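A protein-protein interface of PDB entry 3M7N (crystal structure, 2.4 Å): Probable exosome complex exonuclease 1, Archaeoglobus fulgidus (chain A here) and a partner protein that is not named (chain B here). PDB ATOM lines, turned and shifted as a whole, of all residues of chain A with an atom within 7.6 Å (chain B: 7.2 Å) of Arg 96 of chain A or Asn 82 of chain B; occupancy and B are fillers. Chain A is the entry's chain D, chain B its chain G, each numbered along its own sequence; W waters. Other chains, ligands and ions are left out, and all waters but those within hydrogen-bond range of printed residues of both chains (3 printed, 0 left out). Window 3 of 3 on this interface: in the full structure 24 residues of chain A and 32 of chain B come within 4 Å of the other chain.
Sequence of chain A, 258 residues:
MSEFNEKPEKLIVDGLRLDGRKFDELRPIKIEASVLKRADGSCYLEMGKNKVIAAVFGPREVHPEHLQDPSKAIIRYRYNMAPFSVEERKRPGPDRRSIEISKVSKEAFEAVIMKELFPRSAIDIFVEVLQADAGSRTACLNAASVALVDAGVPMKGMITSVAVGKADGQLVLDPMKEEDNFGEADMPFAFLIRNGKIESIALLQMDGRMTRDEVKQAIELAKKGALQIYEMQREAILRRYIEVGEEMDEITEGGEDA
The guanidinium group (NH2) of Arg 96 of chain A lies close to the side-chain amide nitrogen (ND2) of Asn 82 of chain B (3.4 Å).
The side-chain carboxylate of Glu 100 of chain A is in salt-bridge range of the guanidinium group of Arg 107 of chain B (3.8 Å).
O of Val 81 of chain B lies within hydrogen-bond range of NH2 of Arg 96 of chain A.
OE1 of Glu 100 of chain A lies close to OE1 of Glu 104 of chain B, at 2.7 Å.
The side-chain carboxylate (OD1) of Asp 95 of chain A lies within hydrogen-bond range of the backbone NH (N) of Arg 97 of chain A (3.3 Å).
The backbone NH of Asn 82 of chain B is in hydrogen-bond range of the backbone carbonyl oxygen of Val 137 of chain B, at 2.9 Å.
The backbone carbonyl oxygen (O) of Asn 82 of chain B lies within hydrogen-bond range of the backbone NH (N) of Ile 139 of chain B (2.9 Å).
Among the printed residues, pairs that only touch across the chains: Arg 96 of chain A with Ile 103 of chain B, Arg 96 of chain A with Ala 106 of chain B, Arg 97 of chain A with Arg 107 of chain B and Ile 99 of chain A with Ile 103 of chain B.
Lys 90 of chain A touches none of the printed residues of chain B.
Arg 96 of chain A touches just these residues of chain B: Val 81, Asn 82, Ile 103 and Ala 106.
Printed residues of chain B within 4 Å of Ile 99 of chain A: Ile 103.
Of the printed residues of chain A, Val 81 of chain B touches Arg 96 (3.2 Å).
Asn 82 of chain B touches just one residue of chain A: Arg 96 (3.4 Å).
Printed residues of chain A within 4 Å of Ile 103 of chain B: Arg 96 and Ile 99.
Printed residues of chain A within 4 Å of Ala 106 of chain B: Arg 96.
Of the printed residues of chain A, Arg 107 of chain B touches Arg 97 and Glu 100.
Val 137 of chain B touches none of the printed residues of chain A.
The nearest residue of chain B that does not touch Arg 96 of chain A is Arg 107 of chain B (4.2 Å).
The nearest printed residue of chain A that does not touch Asn 82 of chain B is Asp 95 of chain A (10.6 Å).
Of the 11 printed residues of chain A, 4 touch a printed residue of chain B.
Hydrophobic or aromatic side chains of chain A that line the printed part of chain B: Ile 99.
Among the printed residues, Asp or Glu carboxylates within 4 Å of a Lys or Arg side-chain nitrogen of the other chain: Glu 100 of chain A with Arg 107 of chain B.
Water W3 bridges the guanidinium group (NE) of Arg 107 of chain B and the backbone NH (N) of Arg 97 of chain A.
Water W1 lies within hydrogen-bond range of the guanidinium group of Arg 96 of chain A and the backbone carbonyl oxygen of Val 81 of chain B.
Water W2 lies within hydrogen-bond range of NH1 of Arg 96 of chain A, N of Ala 83 of chain B and OG of Ser 102 of chain B.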
ATOM      1  N   LYS A  90       4.510 -17.239  15.012  1.00  0.00           N
ATOM      2  CA  LYS A  90       3.360 -17.660  14.224  1.00  0.00           C
ATOM      3  C   LYS A  90       2.345 -16.531  14.173  1.00  0.00           C
ATOM      4  O   LYS A  90       1.994 -15.966  15.206  1.00  0.00           O
ATOM      5  CB  LYS A  90       2.706 -18.903  14.835  1.00  0.00           C
ATOM      6  CG  LYS A  90       1.690 -19.566  13.919  1.00  0.00           C
ATOM      7  CD  LYS A  90       0.878 -20.655  14.619  1.00  0.00           C
ATOM      8  CE  LYS A  90      -0.244 -21.148  13.688  1.00  0.00           C
ATOM      9  NZ  LYS A  90      -1.227 -22.058  14.355  1.00  0.00           N
ATOM     10  N   GLY A  93      -4.341 -16.054  14.885  1.00  0.00           N
ATOM     11  CA  GLY A  93      -5.594 -16.393  14.244  1.00  0.00           C
ATOM     12  C   GLY A  93      -5.702 -17.853  13.851  1.00  0.00           C
ATOM     13  O   GLY A  93      -4.693 -18.557  13.743  1.00  0.00           O
ATOM     14  N   PRO A  94      -6.941 -18.323  13.657  1.00  0.00           N
ATOM     15  CA  PRO A  94      -7.209 -19.679  13.170  1.00  0.00           C
ATOM     16  C   PRO A  94      -6.362 -20.060  11.951  1.00  0.00           C
ATOM     17  O   PRO A  94      -5.618 -19.254  11.387  1.00  0.00           O
ATOM     18  CB  PRO A  94      -8.698 -19.641  12.847  1.00  0.00           C
ATOM     19  CG  PRO A  94      -9.254 -18.688  13.896  1.00  0.00           C
ATOM     20  CD  PRO A  94      -8.169 -17.644  14.118  1.00  0.00           C
ATOM     21  N   ASP A  95      -6.519 -21.305  11.533  1.00  0.00           N
ATOM     22  CA  ASP A  95      -5.409 -22.058  11.016  1.00  0.00           C
ATOM     23  C   ASP A  95      -5.955 -23.475  10.879  1.00  0.00           C
ATOM     24  O   ASP A  95      -6.727 -23.928  11.724  1.00  0.00           O
ATOM     25  CB  ASP A  95      -4.330 -21.950  12.090  1.00  0.00           C
ATOM     26  CG  ASP A  95      -3.255 -22.975  11.962  1.00  0.00           C
ATOM     27  OD1 ASP A  95      -3.349 -23.992  12.678  1.00  0.00           O
ATOM     28  OD2 ASP A  95      -2.300 -22.738  11.191  1.00  0.00           O
ATOM     29  N   ARG A  96      -5.611 -24.165   9.799  1.00  0.00           N
ATOM     30  CA  ARG A  96      -6.238 -25.458   9.521  1.00  0.00           C
ATOM     31  C   ARG A  96      -5.957 -26.479  10.625  1.00  0.00           C
ATOM     32  O   ARG A  96      -6.866 -27.178  11.093  1.00  0.00           O
ATOM     33  CB  ARG A  96      -5.802 -26.017   8.160  1.00  0.00           C
ATOM     34  CG  ARG A  96      -6.265 -25.204   6.959  1.00  0.00           C
ATOM     35  CD  ARG A  96      -5.822 -25.845   5.640  1.00  0.00           C
ATOM     36  NE  ARG A  96      -6.899 -26.629   5.038  1.00  0.00           N
ATOM     37  CZ  ARG A  96      -6.770 -27.376   3.945  1.00  0.00           C
ATOM     38  NH1 ARG A  96      -7.816 -28.056   3.480  1.00  0.00           N
ATOM     39  NH2 ARG A  96      -5.596 -27.450   3.319  1.00  0.00           N
ATOM     40  N   ARG A  97      -4.691 -26.560  11.026  1.00  0.00           N
ATOM     41  CA  ARG A  97      -4.286 -27.511  12.045  1.00  0.00           C
ATOM     42  C   ARG A  97      -5.046 -27.192  13.314  1.00  0.00           C
ATOM     43  O   ARG A  97      -5.646 -28.081  13.916  1.00  0.00           O
ATOM     44  CB  ARG A  97      -2.783 -27.446  12.294  1.00  0.00           C
ATOM     45  CG  ARG A  97      -2.250 -28.627  13.102  1.00  0.00           C
ATOM     46  CD  ARG A  97      -0.788 -28.427  13.467  1.00  0.00           C
ATOM     47  NE  ARG A  97      -0.660 -27.311  14.393  1.00  0.00           N
ATOM     48  CZ  ARG A  97      -0.367 -27.431  15.682  1.00  0.00           C
ATOM     49  NH1 ARG A  97      -0.121 -28.622  16.227  1.00  0.00           N
ATOM     50  NH2 ARG A  97      -0.295 -26.342  16.421  1.00  0.00           N
ATOM     51  N   SER A  98      -5.043 -25.909  13.688  1.00  0.00           N
ATOM     52  CA  SER A  98      -5.755 -25.424  14.872  1.00  0.00           C
ATOM     53  C   SER A  98      -7.228 -25.779  14.836  1.00  0.00           C
ATOM     54  O   SER A  98      -7.784 -26.241  15.839  1.00  0.00           O
ATOM     55  CB  SER A  98      -5.595 -23.908  15.034  1.00  0.00           C
ATOM     56  OG  SER A  98      -4.267 -23.579  15.400  1.00  0.00           O
ATOM     57  N   ILE A  99      -7.859 -25.545  13.685  1.00  0.00           N
ATOM     58  CA  ILE A  99      -9.286 -25.806  13.521  1.00  0.00           C
ATOM     59  C   ILE A  99      -9.528 -27.294  13.697  1.00  0.00           C
ATOM     60  O   ILE A  99     -10.485 -27.704  14.350  1.00  0.00           O
ATOM     61  CB  ILE A  99      -9.788 -25.394  12.110  1.00  0.00           C
ATOM     62  CG1 ILE A  99      -9.650 -23.880  11.881  1.00  0.00           C
ATOM     63  CG2 ILE A  99     -11.219 -25.875  11.892  1.00  0.00           C
ATOM     64  CD1 ILE A  99     -10.426 -23.025  12.859  1.00  0.00           C
ATOM     65  N   GLU A 100      -8.651 -28.099  13.100  1.00  0.00           N
ATOM     66  CA  GLU A 100      -8.751 -29.548  13.201  1.00  0.00           C
ATOM     67  C   GLU A 100      -8.614 -29.982  14.655  1.00  0.00           C
ATOM     68  O   GLU A 100      -9.485 -30.671  15.196  1.00  0.00           O
ATOM     69  CB  GLU A 100      -7.703 -30.220  12.312  1.00  0.00           C
ATOM     70  CG  GLU A 100      -7.114 -31.500  12.870  1.00  0.00           C
ATOM     71  CD  GLU A 100      -8.098 -32.648  12.863  1.00  0.00           C
ATOM     72  OE1 GLU A 100      -8.853 -32.772  11.877  1.00  0.00           O
ATOM     73  OE2 GLU A 100      -8.117 -33.426  13.840  1.00  0.00           O
ATOM     74  N   ILE A 101      -7.531 -29.556  15.294  1.00  0.00           N
ATOM     75  CA  ILE A 101      -7.304 -29.882  16.702  1.00  0.00           C
ATOM     76  C   ILE A 101      -8.484 -29.483  17.595  1.00  0.00           C
ATOM     77  O   ILE A 101      -8.902 -30.263  18.469  1.00  0.00           O
ATOM     78  CB  ILE A 101      -6.000 -29.257  17.227  1.00  0.00           C
ATOM     79  CG1 ILE A 101      -4.779 -29.928  16.581  1.00  0.00           C
ATOM     80  CG2 ILE A 101      -5.945 -29.368  18.736  1.00  0.00           C
ATOM     81  CD1 ILE A 101      -3.495 -29.138  16.752  1.00  0.00           C
ATOM     82  N   SER A 102      -9.035 -28.287  17.377  1.00  0.00           N
ATOM     83  CA  SER A 102     -10.180 -27.843  18.183  1.00  0.00           C
ATOM     84  C   SER A 102     -11.360 -28.775  17.997  1.00  0.00           C
ATOM     85  O   SER A 102     -12.072 -29.068  18.950  1.00  0.00           O
ATOM     86  CB  SER A 102     -10.610 -26.410  17.842  1.00  0.00           C
ATOM     87  OG  SER A 102      -9.530 -25.504  17.944  1.00  0.00           O
ATOM     88  N   VAL B  60     -11.574 -35.388  -8.578  1.00  0.00           N
ATOM     89  CA  VAL B  60     -10.367 -34.808  -8.044  1.00  0.00           C
ATOM     90  C   VAL B  60      -9.494 -34.416  -9.193  1.00  0.00           C
ATOM     91  O   VAL B  60      -9.188 -35.233 -10.057  1.00  0.00           O
ATOM     92  CB  VAL B  60      -9.611 -35.797  -7.128  1.00  0.00           C
ATOM     93  CG1 VAL B  60      -8.291 -35.204  -6.682  1.00  0.00           C
ATOM     94  CG2 VAL B  60     -10.494 -36.179  -5.930  1.00  0.00           C
ATOM     95  N   ILE B  80      -0.125 -30.045  -2.053  1.00  0.00           N
ATOM     96  CA  ILE B  80      -1.169 -29.325  -1.331  1.00  0.00           C
ATOM     97  C   ILE B  80      -2.546 -29.873  -1.686  1.00  0.00           C
ATOM     98  O   ILE B  80      -2.916 -29.901  -2.857  1.00  0.00           O
ATOM     99  CB  ILE B  80      -1.119 -27.813  -1.628  1.00  0.00           C
ATOM    100  CG1 ILE B  80       0.285 -27.272  -1.391  1.00  0.00           C
ATOM    101  CG2 ILE B  80      -2.131 -27.046  -0.779  1.00  0.00           C
ATOM    102  CD1 ILE B  80       0.444 -25.840  -1.803  1.00  0.00           C
ATOM    103  N   VAL B  81      -3.285 -30.312  -0.669  1.00  0.00           N
ATOM    104  CA  VAL B  81      -4.621 -30.880  -0.822  1.00  0.00           C
ATOM    105  C   VAL B  81      -5.720 -29.963  -0.261  1.00  0.00           C
ATOM    106  O   VAL B  81      -5.696 -29.606   0.915  1.00  0.00           O
ATOM    107  CB  VAL B  81      -4.749 -32.217  -0.065  1.00  0.00           C
ATOM    108  CG1 VAL B  81      -6.122 -32.848  -0.327  1.00  0.00           C
ATOM    109  CG2 VAL B  81      -3.640 -33.160  -0.448  1.00  0.00           C
ATOM    110  N   ASN B  82      -6.694 -29.608  -1.098  1.00  0.00           N
ATOM    111  CA  ASN B  82      -7.866 -28.854  -0.649  1.00  0.00           C
ATOM    112  C   ASN B  82      -9.174 -29.533  -1.007  1.00  0.00           C
ATOM    113  O   ASN B  82      -9.217 -30.399  -1.866  1.00  0.00           O
ATOM    114  CB  ASN B  82      -7.854 -27.442  -1.232  1.00  0.00           C
ATOM    115  CG  ASN B  82      -6.916 -26.534  -0.502  1.00  0.00           C
ATOM    116  OD1 ASN B  82      -5.813 -26.224  -0.983  1.00  0.00           O
ATOM    117  ND2 ASN B  82      -7.330 -26.114   0.690  1.00  0.00           N
ATOM    118  N   ALA B  83     -10.250 -29.118  -0.365  1.00  0.00           N
ATOM    119  CA  ALA B  83     -11.563 -29.660  -0.690  1.00  0.00           C
ATOM    120  C   ALA B  83     -12.618 -28.576  -0.689  1.00  0.00           C
ATOM    121  O   ALA B  83     -12.561 -27.617   0.088  1.00  0.00           O
ATOM    122  CB  ALA B  83     -11.957 -30.771   0.288  1.00  0.00           C
ATOM    123  N   GLU B  84     -13.583 -28.738  -1.576  1.00  0.00           N
ATOM    124  CA  GLU B  84     -14.762 -27.909  -1.566  1.00  0.00           C
ATOM    125  C   GLU B  84     -15.935 -28.843  -1.469  1.00  0.00           C
ATOM    126  O   GLU B  84     -16.182 -29.633  -2.379  1.00  0.00           O
ATOM    127  CB  GLU B  84     -14.854 -27.078  -2.843  1.00  0.00           C
ATOM    128  CG  GLU B  84     -13.744 -26.052  -2.997  1.00  0.00           C
ATOM    129  CD  GLU B  84     -13.901 -25.178  -4.245  1.00  0.00           C
ATOM    130  OE1 GLU B  84     -12.864 -24.726  -4.787  1.00  0.00           O
ATOM    131  OE2 GLU B  84     -15.051 -24.943  -4.687  1.00  0.00           O
ATOM    132  N   PRO B  98     -13.881 -22.795   3.221  1.00  0.00           N
ATOM    133  CA  PRO B  98     -13.697 -24.155   3.754  1.00  0.00           C
ATOM    134  C   PRO B  98     -14.046 -24.260   5.246  1.00  0.00           C
ATOM    135  O   PRO B  98     -13.352 -23.694   6.102  1.00  0.00           O
ATOM    136  CB  PRO B  98     -12.205 -24.430   3.520  1.00  0.00           C
ATOM    137  CG  PRO B  98     -11.840 -23.569   2.360  1.00  0.00           C
ATOM    138  CD  PRO B  98     -12.706 -22.333   2.455  1.00  0.00           C
ATOM    139  N   SER B 102     -14.862 -29.818   5.781  1.00  0.00           N
ATOM    140  CA  SER B 102     -14.067 -29.781   4.569  1.00  0.00           C
ATOM    141  C   SER B 102     -12.568 -29.736   4.849  1.00  0.00           C
ATOM    142  O   SER B 102     -11.772 -30.328   4.117  1.00  0.00           O
ATOM    143  CB  SER B 102     -14.478 -28.611   3.687  1.00  0.00           C
ATOM    144  OG  SER B 102     -13.529 -28.451   2.653  1.00  0.00           O
ATOM    145  N   ILE B 103     -12.174 -29.029   5.901  1.00  0.00           N
ATOM    146  CA  ILE B 103     -10.761 -28.967   6.247  1.00  0.00           C
ATOM    147  C   ILE B 103     -10.317 -30.346   6.703  1.00  0.00           C
ATOM    148  O   ILE B 103      -9.241 -30.826   6.343  1.00  0.00           O
ATOM    149  CB  ILE B 103     -10.480 -27.946   7.365  1.00  0.00           C
ATOM    150  CG1 ILE B 103     -10.766 -26.520   6.868  1.00  0.00           C
ATOM    151  CG2 ILE B 103      -9.035 -28.070   7.819  1.00  0.00           C
ATOM    152  CD1 ILE B 103     -10.946 -25.508   7.968  1.00  0.00           C
ATOM    153  N   GLU B 104     -11.172 -30.989   7.486  1.00  0.00           N
ATOM    154  CA  GLU B 104     -10.865 -32.304   8.005  1.00  0.00           C
ATOM    155  C   GLU B 104     -10.743 -33.344   6.878  1.00  0.00           C
ATOM    156  O   GLU B 104      -9.777 -34.124   6.830  1.00  0.00           O
ATOM    157  CB  GLU B 104     -11.910 -32.720   9.042  1.00  0.00           C
ATOM    158  CG  GLU B 104     -11.545 -34.003   9.738  1.00  0.00           C
ATOM    159  CD  GLU B 104     -11.980 -34.040  11.185  1.00  0.00           C
ATOM    160  OE1 GLU B 104     -11.099 -34.204  12.050  1.00  0.00           O
ATOM    161  OE2 GLU B 104     -13.193 -33.905  11.461  1.00  0.00           O
ATOM    162  N   LEU B 105     -11.712 -33.350   5.964  1.00  0.00           N
ATOM    163  CA  LEU B 105     -11.684 -34.312   4.867  1.00  0.00           C
ATOM    164  C   LEU B 105     -10.400 -34.153   4.089  1.00  0.00           C
ATOM    165  O   LEU B 105      -9.719 -35.126   3.794  1.00  0.00           O
ATOM    166  CB  LEU B 105     -12.885 -34.138   3.944  1.00  0.00           C
ATOM    167  CG  LEU B 105     -13.072 -35.232   2.884  1.00  0.00           C
ATOM    168  CD1 LEU B 105     -14.561 -35.550   2.671  1.00  0.00           C
ATOM    169  CD2 LEU B 105     -12.379 -34.851   1.589  1.00  0.00           C
ATOM    170  N   ALA B 106     -10.048 -32.916   3.770  1.00  0.00           N
ATOM    171  CA  ALA B 106      -8.869 -32.692   2.951  1.00  0.00           C
ATOM    172  C   ALA B 106      -7.569 -33.071   3.671  1.00  0.00           C
ATOM    173  O   ALA B 106      -6.632 -33.576   3.049  1.00  0.00           O
ATOM    174  CB  ALA B 106      -8.825 -31.260   2.460  1.00  0.00           C
ATOM    175  N   ARG B 107      -7.507 -32.833   4.977  1.00  0.00           N
ATOM    176  CA  ARG B 107      -6.307 -33.180   5.734  1.00  0.00           C
ATOM    177  C   ARG B 107      -6.127 -34.697   5.824  1.00  0.00           C
ATOM    178  O   ARG B 107      -5.006 -35.197   5.710  1.00  0.00           O
ATOM    179  CB  ARG B 107      -6.300 -32.523   7.123  1.00  0.00           C
ATOM    180  CG  ARG B 107      -6.117 -31.014   7.080  1.00  0.00           C
ATOM    181  CD  ARG B 107      -6.222 -30.391   8.458  1.00  0.00           C
ATOM    182  NE  ARG B 107      -4.918 -30.270   9.117  1.00  0.00           N
ATOM    183  CZ  ARG B 107      -4.527 -30.996  10.164  1.00  0.00           C
ATOM    184  NH1 ARG B 107      -3.323 -30.805  10.692  1.00  0.00           N
ATOM    185  NH2 ARG B 107      -5.338 -31.916  10.687  1.00  0.00           N
ATOM    186  N   ASP B 110      -4.789 -35.867   2.604  1.00  0.00           N
ATOM    187  CA  ASP B 110      -3.394 -35.453   2.529  1.00  0.00           C
ATOM    188  C   ASP B 110      -2.442 -36.377   3.302  1.00  0.00           C
ATOM    189  O   ASP B 110      -1.350 -36.702   2.822  1.00  0.00           O
ATOM    190  CB  ASP B 110      -3.239 -34.032   3.053  1.00  0.00           C
ATOM    191  CG  ASP B 110      -1.797 -33.670   3.287  1.00  0.00           C
ATOM    192  OD1 ASP B 110      -1.181 -33.059   2.376  1.00  0.00           O
ATOM    193  OD2 ASP B 110      -1.274 -34.012   4.381  1.00  0.00           O
ATOM    194  N   PHE B 136      -0.875 -29.383  -6.644  1.00  0.00           N
ATOM    195  CA  PHE B 136      -2.192 -29.048  -6.120  1.00  0.00           C
ATOM    196  C   PHE B 136      -3.156 -30.192  -6.375  1.00  0.00           C
ATOM    197  O   PHE B 136      -3.360 -30.608  -7.524  1.00  0.00           O
ATOM    198  CB  PHE B 136      -2.735 -27.791  -6.786  1.00  0.00           C
ATOM    199  CG  PHE B 136      -1.962 -26.548  -6.468  1.00  0.00           C
ATOM    200  CD1 PHE B 136      -1.027 -26.047  -7.368  1.00  0.00           C
ATOM    201  CD2 PHE B 136      -2.178 -25.870  -5.277  1.00  0.00           C
ATOM    202  CE1 PHE B 136      -0.321 -24.889  -7.093  1.00  0.00           C
ATOM    203  CE2 PHE B 136      -1.470 -24.717  -4.988  1.00  0.00           C
ATOM    204  CZ  PHE B 136      -0.541 -24.223  -5.898  1.00  0.00           C
ATOM    205  N   VAL B 137      -3.730 -30.710  -5.297  1.00  0.00           N
ATOM    206  CA  VAL B 137      -4.729 -31.761  -5.375  1.00  0.00           C
ATOM    207  C   VAL B 137      -6.022 -31.171  -4.883  1.00  0.00           C
ATOM    208  O   VAL B 137      -6.173 -30.880  -3.697  1.00  0.00           O
ATOM    209  CB  VAL B 137      -4.363 -32.982  -4.494  1.00  0.00           C
ATOM    210  CG1 VAL B 137      -5.553 -33.925  -4.348  1.00  0.00           C
ATOM    211  CG2 VAL B 137      -3.158 -33.708  -5.071  1.00  0.00           C
ATOM    212  N   ASP B 138      -6.961 -30.974  -5.789  1.00  0.00           N
ATOM    213  CA  ASP B 138      -8.217 -30.359  -5.391  1.00  0.00           C
ATOM    214  C   ASP B 138      -9.400 -31.299  -5.495  1.00  0.00           C
ATOM    215  O   ASP B 138      -9.636 -31.940  -6.526  1.00  0.00           O
ATOM    216  CB  ASP B 138      -8.440 -29.067  -6.157  1.00  0.00           C
ATOM    217  CG  ASP B 138      -7.563 -27.952  -5.650  1.00  0.00           C
ATOM    218  OD1 ASP B 138      -6.507 -27.700  -6.257  1.00  0.00           O
ATOM    219  OD2 ASP B 138      -7.925 -27.343  -4.620  1.00  0.00           O
ATOM    220  N   ILE B 139     -10.130 -31.389  -4.396  1.00  0.00           N
ATOM    221  CA  ILE B 139     -11.232 -32.318  -4.284  1.00  0.00           C
ATOM    222  C   ILE B 139     -12.554 -31.593  -4.423  1.00  0.00           C
ATOM    223  O   ILE B 139     -12.824 -30.635  -3.711  1.00  0.00           O
ATOM    224  CB  ILE B 139     -11.184 -33.021  -2.924  1.00  0.00           C
ATOM    225  CG1 ILE B 139      -9.877 -33.800  -2.804  1.00  0.00           C
ATOM    226  CG2 ILE B 139     -12.400 -33.913  -2.732  1.00  0.00           C
ATOM    227  CD1 ILE B 139      -9.310 -33.809  -1.431  1.00  0.00           C
ATOM    228  N   HIS B 140     -13.384 -32.065  -5.341  1.00  0.00           N
ATOM    229  CA  HIS B 140     -14.678 -31.444  -5.576  1.00  0.00           C
ATOM    230  C   HIS B 140     -15.792 -32.461  -5.444  1.00  0.00           C
ATOM    231  O   HIS B 140     -15.942 -33.346  -6.281  1.00  0.00           O
ATOM    232  CB  HIS B 140     -14.709 -30.788  -6.961  1.00  0.00           C
ATOM    233  CG  HIS B 140     -15.448 -29.488  -6.991  1.00  0.00           C
ATOM    234  ND1 HIS B 140     -16.821 -29.415  -7.127  1.00  0.00           N
ATOM    235  CD2 HIS B 140     -15.009 -28.210  -6.880  1.00  0.00           C
ATOM    236  CE1 HIS B 140     -17.194 -28.150  -7.102  1.00  0.00           C
ATOM    237  NE2 HIS B 140     -16.115 -27.397  -6.954  1.00  0.00           N
HETATM  238  O   HOH W   1      -4.875 -30.089   3.703  1.00  0.00           O
HETATM  239  O   HOH W   2     -10.302 -27.808   2.204  1.00  0.00           O
HETATM  240  O   HOH W   3      -2.975 -28.851   9.057  1.00  0.00           O
